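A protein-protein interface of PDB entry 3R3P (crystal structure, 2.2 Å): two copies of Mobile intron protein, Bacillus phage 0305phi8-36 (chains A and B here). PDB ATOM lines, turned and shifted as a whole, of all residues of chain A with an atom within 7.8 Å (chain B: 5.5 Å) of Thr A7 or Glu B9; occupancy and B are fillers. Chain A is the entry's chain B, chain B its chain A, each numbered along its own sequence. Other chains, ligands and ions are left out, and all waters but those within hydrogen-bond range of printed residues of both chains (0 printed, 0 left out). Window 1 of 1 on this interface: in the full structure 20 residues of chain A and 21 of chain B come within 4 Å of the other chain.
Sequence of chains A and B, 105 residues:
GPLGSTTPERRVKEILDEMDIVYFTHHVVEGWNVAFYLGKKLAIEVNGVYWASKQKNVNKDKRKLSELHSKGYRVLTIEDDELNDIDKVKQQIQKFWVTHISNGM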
ATOM      1  N   SER A   5      23.953  12.875  -7.275  1.00  0.00           N
ATOM      2  CA  SER A   5      25.309  12.584  -6.818  1.00  0.00           C
ATOM      3  C   SER A   5      25.323  11.436  -5.811  1.00  0.00           C
ATOM      4  O   SER A   5      26.363  10.819  -5.571  1.00  0.00           O
ATOM      5  CB  SER A   5      25.945  13.835  -6.208  1.00  0.00           C
ATOM      6  OG  SER A   5      25.096  14.408  -5.225  1.00  0.00           O
ATOM      7  N   THR A   6      24.164  11.154  -5.225  1.00  0.00           N
ATOM      8  CA  THR A   6      24.039  10.052  -4.277  1.00  0.00           C
ATOM      9  C   THR A   6      22.964   9.062  -4.716  1.00  0.00           C
ATOM     10  O   THR A   6      21.939   9.451  -5.277  1.00  0.00           O
ATOM     11  CB  THR A   6      23.726  10.559  -2.858  1.00  0.00           C
ATOM     12  OG1 THR A   6      22.579  11.416  -2.896  1.00  0.00           O
ATOM     13  CG2 THR A   6      24.908  11.332  -2.296  1.00  0.00           C
ATOM     14  N   THR A   7      23.208   7.781  -4.460  1.00  0.00           N
ATOM     15  CA  THR A   7      22.262   6.734  -4.822  1.00  0.00           C
ATOM     16  C   THR A   7      20.962   6.886  -4.039  1.00  0.00           C
ATOM     17  O   THR A   7      20.947   7.491  -2.967  1.00  0.00           O
ATOM     18  CB  THR A   7      22.849   5.332  -4.562  1.00  0.00           C
ATOM     19  OG1 THR A   7      23.072   5.159  -3.157  1.00  0.00           O
ATOM     20  CG2 THR A   7      24.163   5.161  -5.306  1.00  0.00           C
ATOM     21  N   PRO A   8      19.862   6.338  -4.577  1.00  0.00           N
ATOM     22  CA  PRO A   8      18.562   6.424  -3.902  1.00  0.00           C
ATOM     23  C   PRO A   8      18.613   5.872  -2.481  1.00  0.00           C
ATOM     24  O   PRO A   8      18.023   6.463  -1.575  1.00  0.00           O
ATOM     25  CB  PRO A   8      17.645   5.564  -4.784  1.00  0.00           C
ATOM     26  CG  PRO A   8      18.564   4.749  -5.643  1.00  0.00           C
ATOM     27  CD  PRO A   8      19.776   5.596  -5.843  1.00  0.00           C
ATOM     28  N   GLU A   9      19.311   4.758  -2.290  1.00  0.00           N
ATOM     29  CA  GLU A   9      19.447   4.162  -0.965  1.00  0.00           C
ATOM     30  C   GLU A   9      20.201   5.091  -0.019  1.00  0.00           C
ATOM     31  O   GLU A   9      19.836   5.237   1.147  1.00  0.00           O
ATOM     32  CB  GLU A   9      20.160   2.812  -1.050  1.00  0.00           C
ATOM     33  CG  GLU A   9      19.422   1.780  -1.881  1.00  0.00           C
ATOM     34  CD  GLU A   9      20.023   0.397  -1.754  1.00  0.00           C
ATOM     35  OE1 GLU A   9      21.094   0.269  -1.126  1.00  0.00           O
ATOM     36  OE2 GLU A   9      19.420  -0.564  -2.276  1.00  0.00           O
ATOM     37  N   ARG A  10      21.257   5.715  -0.531  1.00  0.00           N
ATOM     38  CA  ARG A  10      22.037   6.665   0.251  1.00  0.00           C
ATOM     39  C   ARG A  10      21.151   7.821   0.696  1.00  0.00           C
ATOM     40  O   ARG A  10      21.217   8.264   1.843  1.00  0.00           O
ATOM     41  CB  ARG A  10      23.207   7.199  -0.577  1.00  0.00           C
ATOM     42  CG  ARG A  10      24.173   8.079   0.196  1.00  0.00           C
ATOM     43  CD  ARG A  10      25.168   7.240   0.977  1.00  0.00           C
ATOM     44  NE  ARG A  10      25.859   6.284   0.116  1.00  0.00           N
ATOM     45  CZ  ARG A  10      26.880   6.592  -0.679  1.00  0.00           C
ATOM     46  NH1 ARG A  10      27.334   7.837  -0.728  1.00  0.00           N
ATOM     47  NH2 ARG A  10      27.444   5.654  -1.428  1.00  0.00           N
ATOM     48  N   ARG A  11      20.318   8.304  -0.223  1.00  0.00           N
ATOM     49  CA  ARG A  11      19.416   9.412   0.063  1.00  0.00           C
ATOM     50  C   ARG A  11      18.369   9.028   1.106  1.00  0.00           C
ATOM     51  O   ARG A  11      18.005   9.840   1.957  1.00  0.00           O
ATOM     52  CB  ARG A  11      18.742   9.903  -1.221  1.00  0.00           C
ATOM     53  CG  ARG A  11      19.710  10.486  -2.241  1.00  0.00           C
ATOM     54  CD  ARG A  11      18.995  10.936  -3.507  1.00  0.00           C
ATOM     55  NE  ARG A  11      17.989  11.959  -3.235  1.00  0.00           N
ATOM     56  CZ  ARG A  11      18.236  13.265  -3.216  1.00  0.00           C
ATOM     57  NH1 ARG A  11      19.462  13.712  -3.455  1.00  0.00           N
ATOM     58  NH2 ARG A  11      17.258  14.123  -2.958  1.00  0.00           N
ATOM     59  N   VAL A  12      17.886   7.792   1.040  1.00  0.00           N
ATOM     60  CA  VAL A  12      16.926   7.311   2.027  1.00  0.00           C
ATOM     61  C   VAL A  12      17.586   7.154   3.393  1.00  0.00           C
ATOM     62  O   VAL A  12      16.983   7.459   4.422  1.00  0.00           O
ATOM     63  CB  VAL A  12      16.289   5.974   1.609  1.00  0.00           C
ATOM     64  CG1 VAL A  12      15.494   5.383   2.765  1.00  0.00           C
ATOM     65  CG2 VAL A  12      15.402   6.174   0.391  1.00  0.00           C
ATOM     66  N   LYS A  13      18.829   6.683   3.400  1.00  0.00           N
ATOM     67  CA  LYS A  13      19.572   6.551   4.645  1.00  0.00           C
ATOM     68  C   LYS A  13      19.680   7.893   5.357  1.00  0.00           C
ATOM     69  O   LYS A  13      19.427   7.991   6.557  1.00  0.00           O
ATOM     70  CB  LYS A  13      20.970   5.984   4.402  1.00  0.00           C
ATOM     71  CG  LYS A  13      21.916   6.240   5.564  1.00  0.00           C
ATOM     72  CD  LYS A  13      23.195   5.434   5.456  1.00  0.00           C
ATOM     73  CE  LYS A  13      24.093   5.694   6.658  1.00  0.00           C
ATOM     74  NZ  LYS A  13      25.206   4.712   6.740  1.00  0.00           N
ATOM     75  N   GLU A  14      20.056   8.925   4.607  1.00  0.00           N
ATOM     76  CA  GLU A  14      20.196  10.264   5.162  1.00  0.00           C
ATOM     77  C   GLU A  14      18.899  10.733   5.814  1.00  0.00           C
ATOM     78  O   GLU A  14      18.921  11.386   6.856  1.00  0.00           O
ATOM     79  CB  GLU A  14      20.638  11.249   4.079  1.00  0.00           C
ATOM     80  CG  GLU A  14      21.990  10.919   3.469  1.00  0.00           C
ATOM     81  CD  GLU A  14      22.398  11.902   2.389  1.00  0.00           C
ATOM     82  OE1 GLU A  14      21.659  12.885   2.169  1.00  0.00           O
ATOM     83  OE2 GLU A  14      23.455  11.689   1.759  1.00  0.00           O
ATOM     84  N   THR A  25      20.807  -2.532   7.132  1.00  0.00           N
ATOM     85  CA  THR A  25      20.908  -2.243   5.703  1.00  0.00           C
ATOM     86  C   THR A  25      20.967  -3.526   4.874  1.00  0.00           C
ATOM     87  O   THR A  25      21.621  -4.493   5.263  1.00  0.00           O
ATOM     88  CB  THR A  25      22.138  -1.368   5.385  1.00  0.00           C
ATOM     89  OG1 THR A  25      22.109  -0.185   6.194  1.00  0.00           O
ATOM     90  CG2 THR A  25      22.140  -0.966   3.920  1.00  0.00           C
ATOM     91  N   HIS A  26      20.282  -3.525   3.733  1.00  0.00           N
ATOM     92  CA  HIS A  26      20.218  -4.694   2.861  1.00  0.00           C
ATOM     93  C   HIS A  26      19.892  -5.954   3.653  1.00  0.00           C
ATOM     94  O   HIS A  26      20.588  -6.963   3.548  1.00  0.00           O
ATOM     95  CB  HIS A  26      21.535  -4.883   2.108  1.00  0.00           C
ATOM     96  CG  HIS A  26      21.926  -3.708   1.268  1.00  0.00           C
ATOM     97  ND1 HIS A  26      23.087  -2.996   1.480  1.00  0.00           N
ATOM     98  CD2 HIS A  26      21.313  -3.122   0.213  1.00  0.00           C
ATOM     99  CE1 HIS A  26      23.172  -2.021   0.592  1.00  0.00           C
ATOM    100  NE2 HIS A  26      22.106  -2.076  -0.188  1.00  0.00           N
ATOM    101  N   ALA A  35      15.954  -2.871   1.431  1.00  0.00           N
ATOM    102  CA  ALA A  35      17.006  -1.866   1.549  1.00  0.00           C
ATOM    103  C   ALA A  35      17.242  -1.461   3.001  1.00  0.00           C
ATOM    104  O   ALA A  35      18.382  -1.303   3.434  1.00  0.00           O
ATOM    105  CB  ALA A  35      16.671  -0.647   0.705  1.00  0.00           C
ATOM    106  N   PHE A  36      16.156  -1.288   3.748  1.00  0.00           N
ATOM    107  CA  PHE A  36      16.253  -0.933   5.156  1.00  0.00           C
ATOM    108  C   PHE A  36      15.205  -1.670   5.975  1.00  0.00           C
ATOM    109  O   PHE A  36      14.015  -1.619   5.668  1.00  0.00           O
ATOM    110  CB  PHE A  36      16.097   0.579   5.347  1.00  0.00           C
ATOM    111  CG  PHE A  36      17.136   1.393   4.627  1.00  0.00           C
ATOM    112  CD1 PHE A  36      18.377   1.622   5.198  1.00  0.00           C
ATOM    113  CD2 PHE A  36      16.871   1.928   3.378  1.00  0.00           C
ATOM    114  CE1 PHE A  36      19.334   2.368   4.538  1.00  0.00           C
ATOM    115  CE2 PHE A  36      17.825   2.675   2.710  1.00  0.00           C
ATOM    116  CZ  PHE A  36      19.057   2.897   3.292  1.00  0.00           C
ATOM    117  N   VAL A  46      13.538   0.332  -1.934  1.00  0.00           N
ATOM    118  CA  VAL A  46      13.852   1.360  -2.913  1.00  0.00           C
ATOM    119  C   VAL A  46      13.808   0.783  -4.323  1.00  0.00           C
ATOM    120  O   VAL A  46      14.568  -0.128  -4.652  1.00  0.00           O
ATOM    121  CB  VAL A  46      15.239   1.976  -2.659  1.00  0.00           C
ATOM    122  CG1 VAL A  46      15.652   2.850  -3.832  1.00  0.00           C
ATOM    123  CG2 VAL A  46      15.234   2.773  -1.364  1.00  0.00           C
ATOM    124  N   SER A  53      20.759  -1.374 -14.862  1.00  0.00           N
ATOM    125  CA  SER A  53      20.955  -2.791 -14.572  1.00  0.00           C
ATOM    126  C   SER A  53      19.669  -3.519 -14.186  1.00  0.00           C
ATOM    127  O   SER A  53      19.665  -4.740 -14.033  1.00  0.00           O
ATOM    128  CB  SER A  53      22.007  -2.967 -13.474  1.00  0.00           C
ATOM    129  OG  SER A  53      21.666  -2.223 -12.316  1.00  0.00           O
ATOM    130  N   ASP A  80      12.612   5.801  -6.916  1.00  0.00           N
ATOM    131  CA  ASP A  80      13.792   6.643  -7.059  1.00  0.00           C
ATOM    132  C   ASP A  80      13.418   8.079  -7.417  1.00  0.00           C
ATOM    133  O   ASP A  80      13.974   9.031  -6.867  1.00  0.00           O
ATOM    134  CB  ASP A  80      14.723   6.064  -8.124  1.00  0.00           C
ATOM    135  CG  ASP A  80      15.999   6.865  -8.278  1.00  0.00           C
ATOM    136  OD1 ASP A  80      16.438   7.069  -9.430  1.00  0.00           O
ATOM    137  OD2 ASP A  80      16.565   7.285  -7.247  1.00  0.00           O
ATOM    138  N   LEU A  83      12.355  10.855  -4.911  1.00  0.00           N
ATOM    139  CA  LEU A  83      13.387  11.519  -4.123  1.00  0.00           C
ATOM    140  C   LEU A  83      13.649  12.948  -4.587  1.00  0.00           C
ATOM    141  O   LEU A  83      14.193  13.759  -3.840  1.00  0.00           O
ATOM    142  CB  LEU A  83      14.684  10.710  -4.145  1.00  0.00           C
ATOM    143  CG  LEU A  83      14.626   9.376  -3.399  1.00  0.00           C
ATOM    144  CD1 LEU A  83      15.849   8.531  -3.710  1.00  0.00           C
ATOM    145  CD2 LEU A  83      14.488   9.610  -1.899  1.00  0.00           C
ATOM    146  N   THR B   7      18.854  -2.929  -6.955  1.00  0.00           N
ATOM    147  CA  THR B   7      19.642  -1.709  -7.085  1.00  0.00           C
ATOM    148  C   THR B   7      21.118  -2.045  -7.268  1.00  0.00           C
ATOM    149  O   THR B   7      21.565  -3.120  -6.869  1.00  0.00           O
ATOM    150  CB  THR B   7      19.491  -0.808  -5.847  1.00  0.00           C
ATOM    151  OG1 THR B   7      20.081  -1.451  -4.711  1.00  0.00           O
ATOM    152  CG2 THR B   7      18.024  -0.528  -5.566  1.00  0.00           C
ATOM    153  N   PRO B   8      21.878  -1.126  -7.880  1.00  0.00           N
ATOM    154  CA  PRO B   8      23.321  -1.301  -8.070  1.00  0.00           C
ATOM    155  C   PRO B   8      24.040  -1.707  -6.784  1.00  0.00           C
ATOM    156  O   PRO B   8      24.815  -2.662  -6.795  1.00  0.00           O
ATOM    157  CB  PRO B   8      23.777   0.087  -8.519  1.00  0.00           C
ATOM    158  CG  PRO B   8      22.599   0.631  -9.244  1.00  0.00           C
ATOM    159  CD  PRO B   8      21.389   0.115  -8.508  1.00  0.00           C
ATOM    160  N   GLU B   9      23.784  -0.994  -5.693  1.00  0.00           N
ATOM    161  CA  GLU B   9      24.422  -1.306  -4.418  1.00  0.00           C
ATOM    162  C   GLU B   9      24.110  -2.731  -3.982  1.00  0.00           C
ATOM    163  O   GLU B   9      25.002  -3.477  -3.575  1.00  0.00           O
ATOM    164  CB  GLU B   9      23.983  -0.317  -3.336  1.00  0.00           C
ATOM    165  CG  GLU B   9      24.455   1.104  -3.575  1.00  0.00           C
ATOM    166  CD  GLU B   9      24.122   2.028  -2.424  1.00  0.00           C
ATOM    167  OE1 GLU B   9      23.259   1.664  -1.600  1.00  0.00           O
ATOM    168  OE2 GLU B   9      24.729   3.117  -2.340  1.00  0.00           O
ATOM    169  N   ARG B  10      22.837  -3.100  -4.068  1.00  0.00           N
ATOM    170  CA  ARG B  10      22.399  -4.445  -3.724  1.00  0.00           C
ATOM    171  C   ARG B  10      23.178  -5.486  -4.523  1.00  0.00           C
ATOM    172  O   ARG B  10      23.612  -6.503  -3.980  1.00  0.00           O
ATOM    173  CB  ARG B  10      20.897  -4.588  -3.985  1.00  0.00           C
ATOM    174  CG  ARG B  10      20.314  -5.942  -3.624  1.00  0.00           C
ATOM    175  CD  ARG B  10      18.817  -5.969  -3.891  1.00  0.00           C
ATOM    176  NE  ARG B  10      18.226  -7.278  -3.630  1.00  0.00           N
ATOM    177  CZ  ARG B  10      16.935  -7.555  -3.770  1.00  0.00           C
ATOM    178  NH1 ARG B  10      16.092  -6.612  -4.169  1.00  0.00           N
ATOM    179  NH2 ARG B  10      16.483  -8.775  -3.512  1.00  0.00           N
ATOM    180  N   ARG B  11      23.357  -5.223  -5.814  1.00  0.00           N
ATOM    181  CA  ARG B  11      24.087  -6.136  -6.687  1.00  0.00           C
ATOM    182  C   ARG B  11      25.562  -6.224  -6.310  1.00  0.00           C
ATOM    183  O   ARG B  11      26.151  -7.303  -6.336  1.00  0.00           O
ATOM    184  CB  ARG B  11      23.944  -5.717  -8.153  1.00  0.00           C
ATOM    185  CG  ARG B  11      22.560  -5.959  -8.731  1.00  0.00           C
ATOM    186  CD  ARG B  11      22.541  -5.744 -10.237  1.00  0.00           C
ATOM    187  NE  ARG B  11      21.252  -6.107 -10.819  1.00  0.00           N
ATOM    188  CZ  ARG B  11      20.241  -5.261 -10.983  1.00  0.00           C
ATOM    189  NH1 ARG B  11      20.368  -3.994 -10.611  1.00  0.00           N
ATOM    190  NH2 ARG B  11      19.103  -5.680 -11.519  1.00  0.00           N
ATOM    191  N   VAL B  12      26.156  -5.087  -5.968  1.00  0.00           N
ATOM    192  CA  VAL B  12      27.549  -5.070  -5.538  1.00  0.00           C
ATOM    193  C   VAL B  12      27.705  -5.815  -4.217  1.00  0.00           C
ATOM    194  O   VAL B  12      28.662  -6.564  -4.026  1.00  0.00           O
ATOM    195  CB  VAL B  12      28.089  -3.634  -5.393  1.00  0.00           C
ATOM    196  CG1 VAL B  12      29.450  -3.645  -4.707  1.00  0.00           C
ATOM    197  CG2 VAL B  12      28.173  -2.961  -6.757  1.00  0.00           C
ATOM    198  N   LYS B  13      26.756  -5.611  -3.310  1.00  0.00           N
ATOM    199  CA  LYS B  13      26.764  -6.311  -2.032  1.00  0.00           C
ATOM    200  C   LYS B  13      26.776  -7.821  -2.234  1.00  0.00           C
ATOM    201  O   LYS B  13      27.539  -8.538  -1.585  1.00  0.00           O
ATOM    202  CB  LYS B  13      25.546  -5.927  -1.194  1.00  0.00           C
ATOM    203  CG  LYS B  13      25.460  -6.685   0.120  1.00  0.00           C
ATOM    204  CD  LYS B  13      24.084  -6.576   0.743  1.00  0.00           C
ATOM    205  CE  LYS B  13      24.072  -7.137   2.156  1.00  0.00           C
ATOM    206  NZ  LYS B  13      24.431  -8.575   2.199  1.00  0.00           N
ATOM    207  N   GLU B  14      25.924  -8.299  -3.135  1.00  0.00           N
ATOM    208  CA  GLU B  14      25.812  -9.729  -3.388  1.00  0.00           C
ATOM    209  C   GLU B  14      27.122 -10.309  -3.907  1.00  0.00           C
ATOM    210  O   GLU B  14      27.503 -11.417  -3.542  1.00  0.00           O
ATOM    211  CB  GLU B  14      24.664 -10.025  -4.357  1.00  0.00           C
ATOM    212  CG  GLU B  14      23.289  -9.675  -3.804  1.00  0.00           C
ATOM    213  CD  GLU B  14      22.161 -10.104  -4.721  1.00  0.00           C
ATOM    214  OE1 GLU B  14      22.427 -10.842  -5.692  1.00  0.00           O
ATOM    215  OE2 GLU B  14      21.004  -9.704  -4.469  1.00  0.00           O
ATOM    216  N   HIS B  26      27.522   2.255   3.380  1.00  0.00           N
ATOM    217  CA  HIS B  26      27.325   3.701   3.451  1.00  0.00           C
ATOM    218  C   HIS B  26      28.185   4.297   4.558  1.00  0.00           C
ATOM    219  O   HIS B  26      27.688   5.011   5.429  1.00  0.00           O
ATOM    220  CB  HIS B  26      25.853   4.041   3.691  1.00  0.00           C
ATOM    221  CG  HIS B  26      24.922   3.448   2.679  1.00  0.00           C
ATOM    222  ND1 HIS B  26      25.039   3.690   1.327  1.00  0.00           N
ATOM    223  CD2 HIS B  26      23.853   2.629   2.822  1.00  0.00           C
ATOM    224  CE1 HIS B  26      24.088   3.042   0.681  1.00  0.00           C
ATOM    225  NE2 HIS B  26      23.354   2.389   1.565  1.00  0.00           N
ATOM    226  N   ALA B  35      29.873   3.753  -0.754  1.00  0.00           N
ATOM    227  CA  ALA B  35      28.895   2.674  -0.726  1.00  0.00           C
ATOM    228  C   ALA B  35      29.363   1.524   0.161  1.00  0.00           C
ATOM    229  O   ALA B  35      28.619   1.047   1.015  1.00  0.00           O
ATOM    230  CB  ALA B  35      28.612   2.176  -2.138  1.00  0.00           C
ATOM    231  N   PHE B  36      30.599   1.085  -0.050  1.00  0.00           N
ATOM    232  CA  PHE B  36      31.163  -0.014   0.726  1.00  0.00           C
ATOM    233  C   PHE B  36      32.603   0.275   1.132  1.00  0.00           C
ATOM    234  O   PHE B  36      33.451   0.558   0.287  1.00  0.00           O
ATOM    235  CB  PHE B  36      31.104  -1.321  -0.072  1.00  0.00           C
ATOM    236  CG  PHE B  36      29.712  -1.739  -0.453  1.00  0.00           C
ATOM    237  CD1 PHE B  36      28.917  -2.442   0.437  1.00  0.00           C
ATOM    238  CD2 PHE B  36      29.202  -1.439  -1.706  1.00  0.00           C
ATOM    239  CE1 PHE B  36      27.636  -2.830   0.087  1.00  0.00           C
ATOM    240  CE2 PHE B  36      27.922  -1.826  -2.062  1.00  0.00           C
ATOM    241  CZ  PHE B  36      27.138  -2.522  -1.165  1.00  0.00           C
ATOM    242  N   VAL B  46      29.477   3.168  -6.087  1.00  0.00           N
ATOM    243  CA  VAL B  46      28.602   2.824  -7.196  1.00  0.00           C
ATOM    244  C   VAL B  46      28.084   4.099  -7.848  1.00  0.00           C
ATOM    245  O   VAL B  46      27.535   4.973  -7.178  1.00  0.00           O
ATOM    246  CB  VAL B  46      27.421   1.947  -6.743  1.00  0.00           C
ATOM    247  CG1 VAL B  46      27.922   0.592  -6.273  1.00  0.00           C
ATOM    248  CG2 VAL B  46      26.640   2.639  -5.641  1.00  0.00           C
ATOM    249  N   TRP B  51      20.396   8.551 -13.149  1.00  0.00           N
ATOM    250  CA  TRP B  51      19.209   7.928 -12.578  1.00  0.00           C
ATOM    251  C   TRP B  51      18.241   9.028 -12.148  1.00  0.00           C
ATOM    252  O   TRP B  51      18.636  10.183 -11.993  1.00  0.00           O
ATOM    253  CB  TRP B  51      19.556   6.987 -11.420  1.00  0.00           C
ATOM    254  CG  TRP B  51      20.357   7.613 -10.321  1.00  0.00           C
ATOM    255  CD1 TRP B  51      19.882   8.358  -9.282  1.00  0.00           C
ATOM    256  CD2 TRP B  51      21.776   7.528 -10.140  1.00  0.00           C
ATOM    257  NE1 TRP B  51      20.919   8.752  -8.469  1.00  0.00           N
ATOM    258  CE2 TRP B  51      22.092   8.255  -8.975  1.00  0.00           C
ATOM    259  CE3 TRP B  51      22.810   6.913 -10.852  1.00  0.00           C
ATOM    260  CZ2 TRP B  51      23.399   8.384  -8.506  1.00  0.00           C
ATOM    261  CZ3 TRP B  51      24.106   7.041 -10.386  1.00  0.00           C
ATOM    262  CH2 TRP B  51      24.389   7.771  -9.223  1.00  0.00           C
ATOM    263  N   SER B  53      16.807  10.368  -9.581  1.00  0.00           N
ATOM    264  CA  SER B  53      17.087  11.333  -8.522  1.00  0.00           C
ATOM    265  C   SER B  53      18.553  11.757  -8.468  1.00  0.00           C
ATOM    266  O   SER B  53      19.011  12.292  -7.460  1.00  0.00           O
ATOM    267  CB  SER B  53      16.669  10.770  -7.163  1.00  0.00           C
ATOM    268  OG  SER B  53      17.484   9.669  -6.801  1.00  0.00           O
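The side-chain hydroxyl (OG1) of Thr B7 lies within hydrogen-bond range of the side-chain carboxylate (OE2) of Glu A9, 2.7 Å away. The side-chain hydroxyl (OG1) of Thr A7 lies within hydrogen-bond range of the side-chain carboxylate (OE2) of Glu B9, 2.8 Å away. The side-chain carboxylate (OE1) of Glu B9 sits close to the side-chain carboxylate (OE1) of Glu A9 (2.6 Å). OE2 of Glu B9 lies within salt-bridge range of NH2 of Arg A10. NH2 of Arg B11 sits at hydrogen-bond distance from O of Ser A53. ND1 of His B26 sits at hydrogen-bond distance from NE of Arg A10. NZ of Lys A13 lies within hydrogen-bond range of O of His B26 (2.8 Å). The indole nitrogen (NE1) of Trp B51 is in hydrogen-bond range of the backbone carbonyl oxygen (O) of Thr A6 (3.4 Å). The side-chain carboxylate of Asp A80 lies within hydrogen-bond range of the side-chain hydroxyl of Ser B53 (2.6 Å). The guanidinium group (NH2) of Arg A10 lies close to the backbone NH (N) of Ala B35 (3.2 Å).
Hydrophobic or aromatic side chains of chain A that line the printed part of chain B: His A26 and Leu A83. Hydrophobic or aromatic side chains of chain B within 4 Å of the printed part of chain A: His B26, Ala B35, Val B46 and Trp B51. Along chain B the printed residues that touch a printed residue of chain A span positions 7 to 53.
Arg A10 touches His B26, but with the chains exchanged His A26 does not touch Arg B10 (4.1 Å). Arg A10 touches Ala B35, but with the chains exchanged Ala A35 does not touch Arg B10 (6.7 Å). Arg A11 touches Ser B53, and with the chains exchanged Ser A53 touches Arg B11. Lys A13 touches His B26, and with the chains exchanged His A26 touches Lys B13. 13 positions are printed for both chains.
Thr A7 touches two residues of chain B. Pro A8 touches none of the printed residues of chain B. Printed residues of chain B within 4 Å of Glu A9: Thr B7 and Glu B9. Ala A35 touches none of the printed residues of chain B. Of the printed residues of chain B, Asp A80 touches Trp B51 (3.7 Å) and Ser B53 (2.6 Å). Glu B9 touches just these residues of chain A: Thr A7 (2.8 Å), Glu A9 (2.6 Å) and Arg A10 (3.8 Å). The nearest residue of chain A that does not touch Glu B9 is His A26 (4.1 Å).
Among the printed residues, pairs that only touch across the chains: Thr A7 with Val B46, Arg A11 with Ser B53, His A26 with Lys B13, Val A46 with Thr B7, Asp A80 with Trp B51 and Leu A83 with Ser B53.
The side-chain hydroxyl of Thr B7 is in hydrogen-bond range of the backbone NH of Arg B10. N of His B26 sits at hydrogen-bond distance from O of Ala B35 (2.9 Å). OG1 of Thr A7 sits at hydrogen-bond distance from N of Arg A10 (3.2 Å). A ring nitrogen (NE2) of His A26 lies within hydrogen-bond range of the side-chain carboxylate (OE1) of Glu A9 (2.7 Å). NH2 of Arg A11 sits at hydrogen-bond distance from O of Leu A83 (3.2 Å). O of Ala A35 sits at hydrogen-bond distance from N of His A26 (2.9 Å).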
